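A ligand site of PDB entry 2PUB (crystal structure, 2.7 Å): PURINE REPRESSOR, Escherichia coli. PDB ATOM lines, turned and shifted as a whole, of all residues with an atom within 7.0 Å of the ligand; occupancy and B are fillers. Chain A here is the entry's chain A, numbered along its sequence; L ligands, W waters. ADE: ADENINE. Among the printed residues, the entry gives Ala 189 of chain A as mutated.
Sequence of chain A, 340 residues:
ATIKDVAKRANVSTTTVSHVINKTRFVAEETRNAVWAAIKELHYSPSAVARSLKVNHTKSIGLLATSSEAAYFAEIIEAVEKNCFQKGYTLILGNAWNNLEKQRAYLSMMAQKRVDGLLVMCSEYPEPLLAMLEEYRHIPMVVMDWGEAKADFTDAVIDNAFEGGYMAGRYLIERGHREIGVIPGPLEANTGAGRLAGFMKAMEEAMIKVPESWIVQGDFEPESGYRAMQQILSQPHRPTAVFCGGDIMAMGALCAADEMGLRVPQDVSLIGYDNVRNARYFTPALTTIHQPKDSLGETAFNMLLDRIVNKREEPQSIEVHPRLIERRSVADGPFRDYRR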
ATOM      1  N   THR A  66      21.132   6.445  19.751  1.00  0.00           N
ATOM      2  CA  THR A  66      20.273   5.284  19.918  1.00  0.00           C
ATOM      3  C   THR A  66      21.097   4.029  20.011  1.00  0.00           C
ATOM      4  O   THR A  66      20.937   3.227  20.850  1.00  0.00           O
ATOM      5  CB  THR A  66      19.342   5.115  18.727  1.00  0.00           C
ATOM      6  OG1 THR A  66      18.196   5.977  18.863  1.00  0.00           O
ATOM      7  CG2 THR A  66      18.930   3.675  18.654  1.00  0.00           C
ATOM      8  N   SER A  67      22.010   3.867  19.087  1.00  0.00           N
ATOM      9  CA  SER A  67      22.854   2.691  19.068  1.00  0.00           C
ATOM     10  C   SER A  67      24.094   3.071  18.259  1.00  0.00           C
ATOM     11  O   SER A  67      24.047   3.946  17.421  1.00  0.00           O
ATOM     12  CB  SER A  67      22.115   1.498  18.420  1.00  0.00           C
ATOM     13  OG  SER A  67      22.792   1.033  17.271  1.00  0.00           O
ATOM     14  N   ALA A  70      24.794   0.151  14.393  1.00  0.00           N
ATOM     15  CA  ALA A  70      24.183   0.468  13.083  1.00  0.00           C
ATOM     16  C   ALA A  70      25.081   1.307  12.180  1.00  0.00           C
ATOM     17  O   ALA A  70      25.556   2.397  12.554  1.00  0.00           O
ATOM     18  CB  ALA A  70      22.810   1.183  13.295  1.00  0.00           C
ATOM     19  N   ALA A  71      25.356   0.726  11.030  1.00  0.00           N
ATOM     20  CA  ALA A  71      26.196   1.339  10.003  1.00  0.00           C
ATOM     21  C   ALA A  71      25.940   2.849   9.894  1.00  0.00           C
ATOM     22  O   ALA A  71      26.851   3.663  10.015  1.00  0.00           O
ATOM     23  CB  ALA A  71      25.926   0.644   8.671  1.00  0.00           C
ATOM     24  N   TYR A  72      24.662   3.152   9.687  1.00  0.00           N
ATOM     25  CA  TYR A  72      24.167   4.490   9.549  1.00  0.00           C
ATOM     26  C   TYR A  72      24.783   5.336  10.658  1.00  0.00           C
ATOM     27  O   TYR A  72      25.721   6.079  10.458  1.00  0.00           O
ATOM     28  CB  TYR A  72      22.656   4.409   9.668  1.00  0.00           C
ATOM     29  CG  TYR A  72      21.971   5.727   9.506  1.00  0.00           C
ATOM     30  CD1 TYR A  72      22.143   6.464   8.371  1.00  0.00           C
ATOM     31  CD2 TYR A  72      21.145   6.223  10.480  1.00  0.00           C
ATOM     32  CE1 TYR A  72      21.516   7.688   8.199  1.00  0.00           C
ATOM     33  CE2 TYR A  72      20.509   7.441  10.315  1.00  0.00           C
ATOM     34  CZ  TYR A  72      20.716   8.154   9.164  1.00  0.00           C
ATOM     35  OH  TYR A  72      20.142   9.363   8.951  1.00  0.00           O
ATOM     36  N   PHE A  73      24.290   5.112  11.842  1.00  0.00           N
ATOM     37  CA  PHE A  73      24.745   5.767  13.030  1.00  0.00           C
ATOM     38  C   PHE A  73      26.197   5.855  13.161  1.00  0.00           C
ATOM     39  O   PHE A  73      26.796   6.914  13.387  1.00  0.00           O
ATOM     40  CB  PHE A  73      24.234   4.972  14.193  1.00  0.00           C
ATOM     41  CG  PHE A  73      22.794   5.162  14.361  1.00  0.00           C
ATOM     42  CD1 PHE A  73      22.304   6.447  14.287  1.00  0.00           C
ATOM     43  CD2 PHE A  73      21.936   4.082  14.419  1.00  0.00           C
ATOM     44  CE1 PHE A  73      20.976   6.685  14.366  1.00  0.00           C
ATOM     45  CE2 PHE A  73      20.577   4.318  14.496  1.00  0.00           C
ATOM     46  CZ  PHE A  73      20.095   5.618  14.458  1.00  0.00           C
ATOM     47  N   ASN A  98      16.554   3.674  22.774  1.00  0.00           N
ATOM     48  CA  ASN A  98      15.125   3.999  22.804  1.00  0.00           C
ATOM     49  C   ASN A  98      14.462   3.599  24.123  1.00  0.00           C
ATOM     50  O   ASN A  98      13.280   3.311  24.155  1.00  0.00           O
ATOM     51  CB  ASN A  98      14.376   3.291  21.667  1.00  0.00           C
ATOM     52  CG  ASN A  98      14.261   4.130  20.456  1.00  0.00           C
ATOM     53  OD1 ASN A  98      14.795   3.794  19.402  1.00  0.00           O
ATOM     54  ND2 ASN A  98      13.585   5.266  20.588  1.00  0.00           N
ATOM     55  N   SER A 123      16.072   8.822  17.305  1.00  0.00           N
ATOM     56  CA  SER A 123      15.176   8.126  16.425  1.00  0.00           C
ATOM     57  C   SER A 123      13.711   8.374  16.709  1.00  0.00           C
ATOM     58  O   SER A 123      13.048   8.975  15.913  1.00  0.00           O
ATOM     59  CB  SER A 123      15.548   6.640  16.361  1.00  0.00           C
ATOM     60  OG  SER A 123      15.801   6.272  15.010  1.00  0.00           O
ATOM     61  N   ASP A 145      18.014  14.577  14.206  1.00  0.00           N
ATOM     62  CA  ASP A 145      17.139  13.701  13.452  1.00  0.00           C
ATOM     63  C   ASP A 145      15.632  13.942  13.436  1.00  0.00           C
ATOM     64  O   ASP A 145      14.840  13.000  13.376  1.00  0.00           O
ATOM     65  CB  ASP A 145      17.494  12.228  13.748  1.00  0.00           C
ATOM     66  CG  ASP A 145      17.248  11.840  15.229  1.00  0.00           C
ATOM     67  OD1 ASP A 145      16.675  12.667  15.974  1.00  0.00           O
ATOM     68  OD2 ASP A 145      17.551  10.687  15.609  1.00  0.00           O
ATOM     69  N   PRO A 186      10.523   1.886  10.791  1.00  0.00           N
ATOM     70  CA  PRO A 186       9.575   2.265  11.844  1.00  0.00           C
ATOM     71  C   PRO A 186       8.902   3.620  11.614  1.00  0.00           C
ATOM     72  O   PRO A 186       9.524   4.647  11.403  1.00  0.00           O
ATOM     73  CB  PRO A 186      10.451   2.295  13.099  1.00  0.00           C
ATOM     74  CG  PRO A 186      11.831   1.853  12.687  1.00  0.00           C
ATOM     75  CD  PRO A 186      11.693   1.178  11.345  1.00  0.00           C
ATOM     76  N   ALA A 189       9.608   6.791  13.599  1.00  0.00           N
ATOM     77  CA  ALA A 189      10.828   7.537  13.312  1.00  0.00           C
ATOM     78  C   ALA A 189      10.658   8.318  12.006  1.00  0.00           C
ATOM     79  O   ALA A 189       9.890   7.943  11.125  1.00  0.00           O
ATOM     80  CB  ALA A 189      12.033   6.593  13.283  1.00  0.00           C
ATOM     81  N   ASN A 190      11.374   9.420  11.880  1.00  0.00           N
ATOM     82  CA  ASN A 190      11.365  10.255  10.696  1.00  0.00           C
ATOM     83  C   ASN A 190      11.872   9.525   9.455  1.00  0.00           C
ATOM     84  O   ASN A 190      11.172   9.413   8.441  1.00  0.00           O
ATOM     85  CB  ASN A 190      12.220  11.494  10.927  1.00  0.00           C
ATOM     86  CG  ASN A 190      12.327  12.380   9.676  1.00  0.00           C
ATOM     87  OD1 ASN A 190      11.299  12.786   9.077  1.00  0.00           O
ATOM     88  ND2 ASN A 190      13.584  12.718   9.285  1.00  0.00           N
ATOM     89  N   THR A 191      13.109   9.052   9.531  1.00  0.00           N
ATOM     90  CA  THR A 191      13.709   8.288   8.430  1.00  0.00           C
ATOM     91  C   THR A 191      12.796   7.129   8.054  1.00  0.00           C
ATOM     92  O   THR A 191      12.945   6.568   6.984  1.00  0.00           O
ATOM     93  CB  THR A 191      15.070   7.739   8.807  1.00  0.00           C
ATOM     94  OG1 THR A 191      14.972   7.095  10.069  1.00  0.00           O
ATOM     95  CG2 THR A 191      16.121   8.831   8.968  1.00  0.00           C
ATOM     96  N   GLY A 192      11.863   6.802   8.948  1.00  0.00           N
ATOM     97  CA  GLY A 192      10.909   5.741   8.675  1.00  0.00           C
ATOM     98  C   GLY A 192       9.692   6.409   7.998  1.00  0.00           C
ATOM     99  O   GLY A 192       9.518   6.415   6.764  1.00  0.00           O
ATOM    100  N   ARG A 195      10.359   8.959   4.891  1.00  0.00           N
ATOM    101  CA  ARG A 195      10.862   8.453   3.652  1.00  0.00           C
ATOM    102  C   ARG A 195       9.669   7.797   2.920  1.00  0.00           C
ATOM    103  O   ARG A 195       9.448   8.010   1.749  1.00  0.00           O
ATOM    104  CB  ARG A 195      12.028   7.489   3.938  1.00  0.00           C
ATOM    105  CG  ARG A 195      13.389   8.204   4.307  1.00  0.00           C
ATOM    106  CD  ARG A 195      14.457   7.163   4.725  1.00  0.00           C
ATOM    107  NE  ARG A 195      15.696   7.774   5.226  1.00  0.00           N
ATOM    108  CZ  ARG A 195      16.757   7.078   5.610  1.00  0.00           C
ATOM    109  NH1 ARG A 195      16.679   5.747   5.562  1.00  0.00           N
ATOM    110  NH2 ARG A 195      17.860   7.714   6.077  1.00  0.00           N
ATOM    111  N   ASP A 219      12.734  -2.623  10.593  1.00  0.00           N
ATOM    112  CA  ASP A 219      13.176  -1.933  11.796  1.00  0.00           C
ATOM    113  C   ASP A 219      14.606  -1.540  11.598  1.00  0.00           C
ATOM    114  O   ASP A 219      15.353  -1.493  12.571  1.00  0.00           O
ATOM    115  CB  ASP A 219      13.084  -2.879  12.998  1.00  0.00           C
ATOM    116  CG  ASP A 219      13.928  -4.122  12.851  1.00  0.00           C
ATOM    117  OD1 ASP A 219      14.757  -4.293  11.917  1.00  0.00           O
ATOM    118  OD2 ASP A 219      13.726  -4.980  13.715  1.00  0.00           O
ATOM    119  N   PHE A 220      14.988  -1.291  10.347  1.00  0.00           N
ATOM    120  CA  PHE A 220      16.371  -0.960   9.979  1.00  0.00           C
ATOM    121  C   PHE A 220      17.368  -2.086  10.162  1.00  0.00           C
ATOM    122  O   PHE A 220      18.542  -1.925   9.819  1.00  0.00           O
ATOM    123  CB  PHE A 220      16.878   0.287  10.672  1.00  0.00           C
ATOM    124  CG  PHE A 220      16.141   1.502  10.283  1.00  0.00           C
ATOM    125  CD1 PHE A 220      16.193   1.962   8.989  1.00  0.00           C
ATOM    126  CD2 PHE A 220      15.360   2.187  11.210  1.00  0.00           C
ATOM    127  CE1 PHE A 220      15.496   3.069   8.604  1.00  0.00           C
ATOM    128  CE2 PHE A 220      14.666   3.306  10.841  1.00  0.00           C
ATOM    129  CZ  PHE A 220      14.745   3.749   9.540  1.00  0.00           C
ATOM    130  N   GLU A 221      16.941  -3.209  10.733  1.00  0.00           N
ATOM    131  CA  GLU A 221      17.870  -4.311  10.916  1.00  0.00           C
ATOM    132  C   GLU A 221      17.756  -5.327   9.752  1.00  0.00           C
ATOM    133  O   GLU A 221      16.672  -5.602   9.220  1.00  0.00           O
ATOM    134  CB  GLU A 221      17.702  -4.942  12.300  1.00  0.00           C
ATOM    135  CG  GLU A 221      18.104  -4.009  13.413  1.00  0.00           C
ATOM    136  CD  GLU A 221      19.469  -4.268  13.970  1.00  0.00           C
ATOM    137  OE1 GLU A 221      20.456  -4.064  13.228  1.00  0.00           O
ATOM    138  OE2 GLU A 221      19.555  -4.741  15.124  1.00  0.00           O
ATOM    139  N   GLY A 245      13.416   1.027   2.809  1.00  0.00           N
ATOM    140  CA  GLY A 245      13.689   2.139   3.711  1.00  0.00           C
ATOM    141  C   GLY A 245      15.091   2.427   4.239  1.00  0.00           C
ATOM    142  O   GLY A 245      15.324   3.508   4.758  1.00  0.00           O
ATOM    143  N   GLY A 246      16.036   1.482   4.127  1.00  0.00           N
ATOM    144  CA  GLY A 246      17.428   1.647   4.622  1.00  0.00           C
ATOM    145  C   GLY A 246      18.367   0.589   4.013  1.00  0.00           C
ATOM    146  O   GLY A 246      17.973  -0.564   3.739  1.00  0.00           O
ATOM    147  N   ASP A 247      19.609   0.960   3.753  1.00  0.00           N
ATOM    148  CA  ASP A 247      20.527   0.023   3.125  1.00  0.00           C
ATOM    149  C   ASP A 247      20.723  -1.361   3.801  1.00  0.00           C
ATOM    150  O   ASP A 247      20.580  -2.427   3.148  1.00  0.00           O
ATOM    151  CB  ASP A 247      21.833   0.745   2.820  1.00  0.00           C
ATOM    152  CG  ASP A 247      21.681   1.787   1.737  1.00  0.00           C
ATOM    153  OD1 ASP A 247      20.567   1.854   1.167  1.00  0.00           O
ATOM    154  OD2 ASP A 247      22.637   2.509   1.422  1.00  0.00           O
ATOM    155  N   ILE A 248      21.003  -1.333   5.098  1.00  0.00           N
ATOM    156  CA  ILE A 248      21.142  -2.572   5.823  1.00  0.00           C
ATOM    157  C   ILE A 248      19.928  -3.523   5.689  1.00  0.00           C
ATOM    158  O   ILE A 248      20.094  -4.723   5.545  1.00  0.00           O
ATOM    159  CB  ILE A 248      21.580  -2.365   7.263  1.00  0.00           C
ATOM    160  CG1 ILE A 248      22.740  -1.393   7.307  1.00  0.00           C
ATOM    161  CG2 ILE A 248      21.959  -3.711   7.853  1.00  0.00           C
ATOM    162  CD1 ILE A 248      24.009  -2.034   6.740  1.00  0.00           C
ATOM    163  N   TYR A 273      18.182   3.065   0.698  1.00  0.00           N
ATOM    164  CA  TYR A 273      18.269   4.398   1.210  1.00  0.00           C
ATOM    165  C   TYR A 273      19.253   4.443   2.313  1.00  0.00           C
ATOM    166  O   TYR A 273      19.169   3.647   3.228  1.00  0.00           O
ATOM    167  CB  TYR A 273      16.958   4.732   1.847  1.00  0.00           C
ATOM    168  CG  TYR A 273      16.769   6.220   1.964  1.00  0.00           C
ATOM    169  CD1 TYR A 273      17.739   7.023   2.495  1.00  0.00           C
ATOM    170  CD2 TYR A 273      15.625   6.808   1.465  1.00  0.00           C
ATOM    171  CE1 TYR A 273      17.563   8.392   2.582  1.00  0.00           C
ATOM    172  CE2 TYR A 273      15.443   8.159   1.528  1.00  0.00           C
ATOM    173  CZ  TYR A 273      16.398   8.951   2.096  1.00  0.00           C
ATOM    174  OH  TYR A 273      16.168  10.282   2.199  1.00  0.00           O
ATOM    175  N   ASP A 274      20.168   5.402   2.190  1.00  0.00           N
ATOM    176  CA  ASP A 274      21.208   5.799   3.149  1.00  0.00           C
ATOM    177  C   ASP A 274      22.553   5.945   2.508  1.00  0.00           C
ATOM    178  O   ASP A 274      23.332   6.861   2.805  1.00  0.00           O
ATOM    179  CB  ASP A 274      21.359   4.842   4.348  1.00  0.00           C
ATOM    180  CG  ASP A 274      20.220   4.998   5.386  1.00  0.00           C
ATOM    181  OD1 ASP A 274      19.461   5.981   5.258  1.00  0.00           O
ATOM    182  OD2 ASP A 274      20.239   4.237   6.400  1.00  0.00           O
ATOM    183  N   VAL A 276      25.121   3.765   2.725  1.00  0.00           N
ATOM    184  CA  VAL A 276      26.094   3.477   3.744  1.00  0.00           C
ATOM    185  C   VAL A 276      27.401   3.173   3.062  1.00  0.00           C
ATOM    186  O   VAL A 276      27.414   2.546   2.024  1.00  0.00           O
ATOM    187  CB  VAL A 276      25.703   2.168   4.467  1.00  0.00           C
ATOM    188  CG1 VAL A 276      26.961   1.369   4.875  1.00  0.00           C
ATOM    189  CG2 VAL A 276      24.841   2.551   5.660  1.00  0.00           C
ATOM    190  N   GLN A 291      22.435   9.774   1.918  1.00  0.00           N
ATOM    191  CA  GLN A 291      22.219  10.711   2.996  1.00  0.00           C
ATOM    192  C   GLN A 291      23.563  11.261   3.375  1.00  0.00           C
ATOM    193  O   GLN A 291      24.487  10.513   3.656  1.00  0.00           O
ATOM    194  CB  GLN A 291      21.605  10.032   4.253  1.00  0.00           C
ATOM    195  CG  GLN A 291      21.490  10.992   5.429  1.00  0.00           C
ATOM    196  CD  GLN A 291      20.060  11.460   5.708  1.00  0.00           C
ATOM    197  OE1 GLN A 291      19.483  11.090   6.743  1.00  0.00           O
ATOM    198  NE2 GLN A 291      19.499  12.313   4.867  1.00  0.00           N
HETATM  199  N9  ADE L   1      18.935   4.787   8.582  1.00  0.00           N
HETATM  200  C8  ADE L   1      17.933   5.712   8.736  1.00  0.00           C
HETATM  201  N7  ADE L   1      17.376   5.673   9.904  1.00  0.00           N
HETATM  202  C5  ADE L   1      17.998   4.635  10.573  1.00  0.00           C
HETATM  203  C6  ADE L   1      17.816   4.091  11.873  1.00  0.00           C
HETATM  204  N6  ADE L   1      16.953   4.506  12.803  1.00  0.00           N
HETATM  205  N1  ADE L   1      18.651   3.025  12.142  1.00  0.00           N
HETATM  206  C2  ADE L   1      19.585   2.536  11.261  1.00  0.00           C
HETATM  207  N3  ADE L   1      19.777   3.029  10.045  1.00  0.00           N
HETATM  208  C4  ADE L   1      18.956   4.068   9.755  1.00  0.00           C
HETATM  209  O   HOH W   1      17.855   1.605  15.006  1.00  0.00           O
HETATM  210  O   HOH W   2      16.256   3.535  15.706  1.00  0.00           O
HETATM  211  O   HOH W   3      22.013   1.547   9.714  1.00  0.00           O
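A nitrogen (N9) of the ligand lies within hydrogen-bond range of the side-chain carboxylate (OD2) of Asp 274, at 2.6 Å.
The side-chain hydroxyl (OG) of Ser 123 lies within hydrogen-bond range of a nitrogen (N6) of the ligand, at 3.1 Å.
OG1 of Thr 191 sits at hydrogen-bond distance from N7 of the ligand, at 2.8 Å.
The side-chain carboxylate of Asp 274 is in salt-bridge range of the guanidinium group of Arg 195 (2.5 Å).
OE1 of Gln 291 sits at hydrogen-bond distance from OH of Tyr 72 (2.9 Å).
The backbone carbonyl oxygen of Thr 191 sits close to the guanidinium group of Arg 195, at 3.5 Å.
The guanidinium group (NH1) of Arg 195 sits at hydrogen-bond distance from the backbone carbonyl oxygen (O) of Gly 245 (2.7 Å).
The backbone NH (N) of Gln 291 sits at hydrogen-bond distance from the backbone carbonyl oxygen (O) of Asp 274, 3.2 Å away.
N of Ser 123 is in hydrogen-bond range of OD2 of Asp 145, 2.9 Å away.
Tyr 72 touches the ligand.
Phe 73 touches the ligand (CE2 to N1, 3.3 Å).
Arg 195 touches the ligand (NH2 to C8, 3.3 Å).
Phe 220 touches the ligand.
Hydrophobic or aromatic side chains within 4 Å of the ligand: Tyr 72, Phe 73 and Phe 220.
The nearest printed residue that does not touch the ligand is Ala 70 (4.05 Å).
Water W3 lies within hydrogen-bond range of a nitrogen (N3) of the ligand and the backbone NH of Tyr 72.
Water W2 lies within hydrogen-bond range of OG of Ser 123 (2.9 Å) and N6 of the ligand (3.1 Å).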
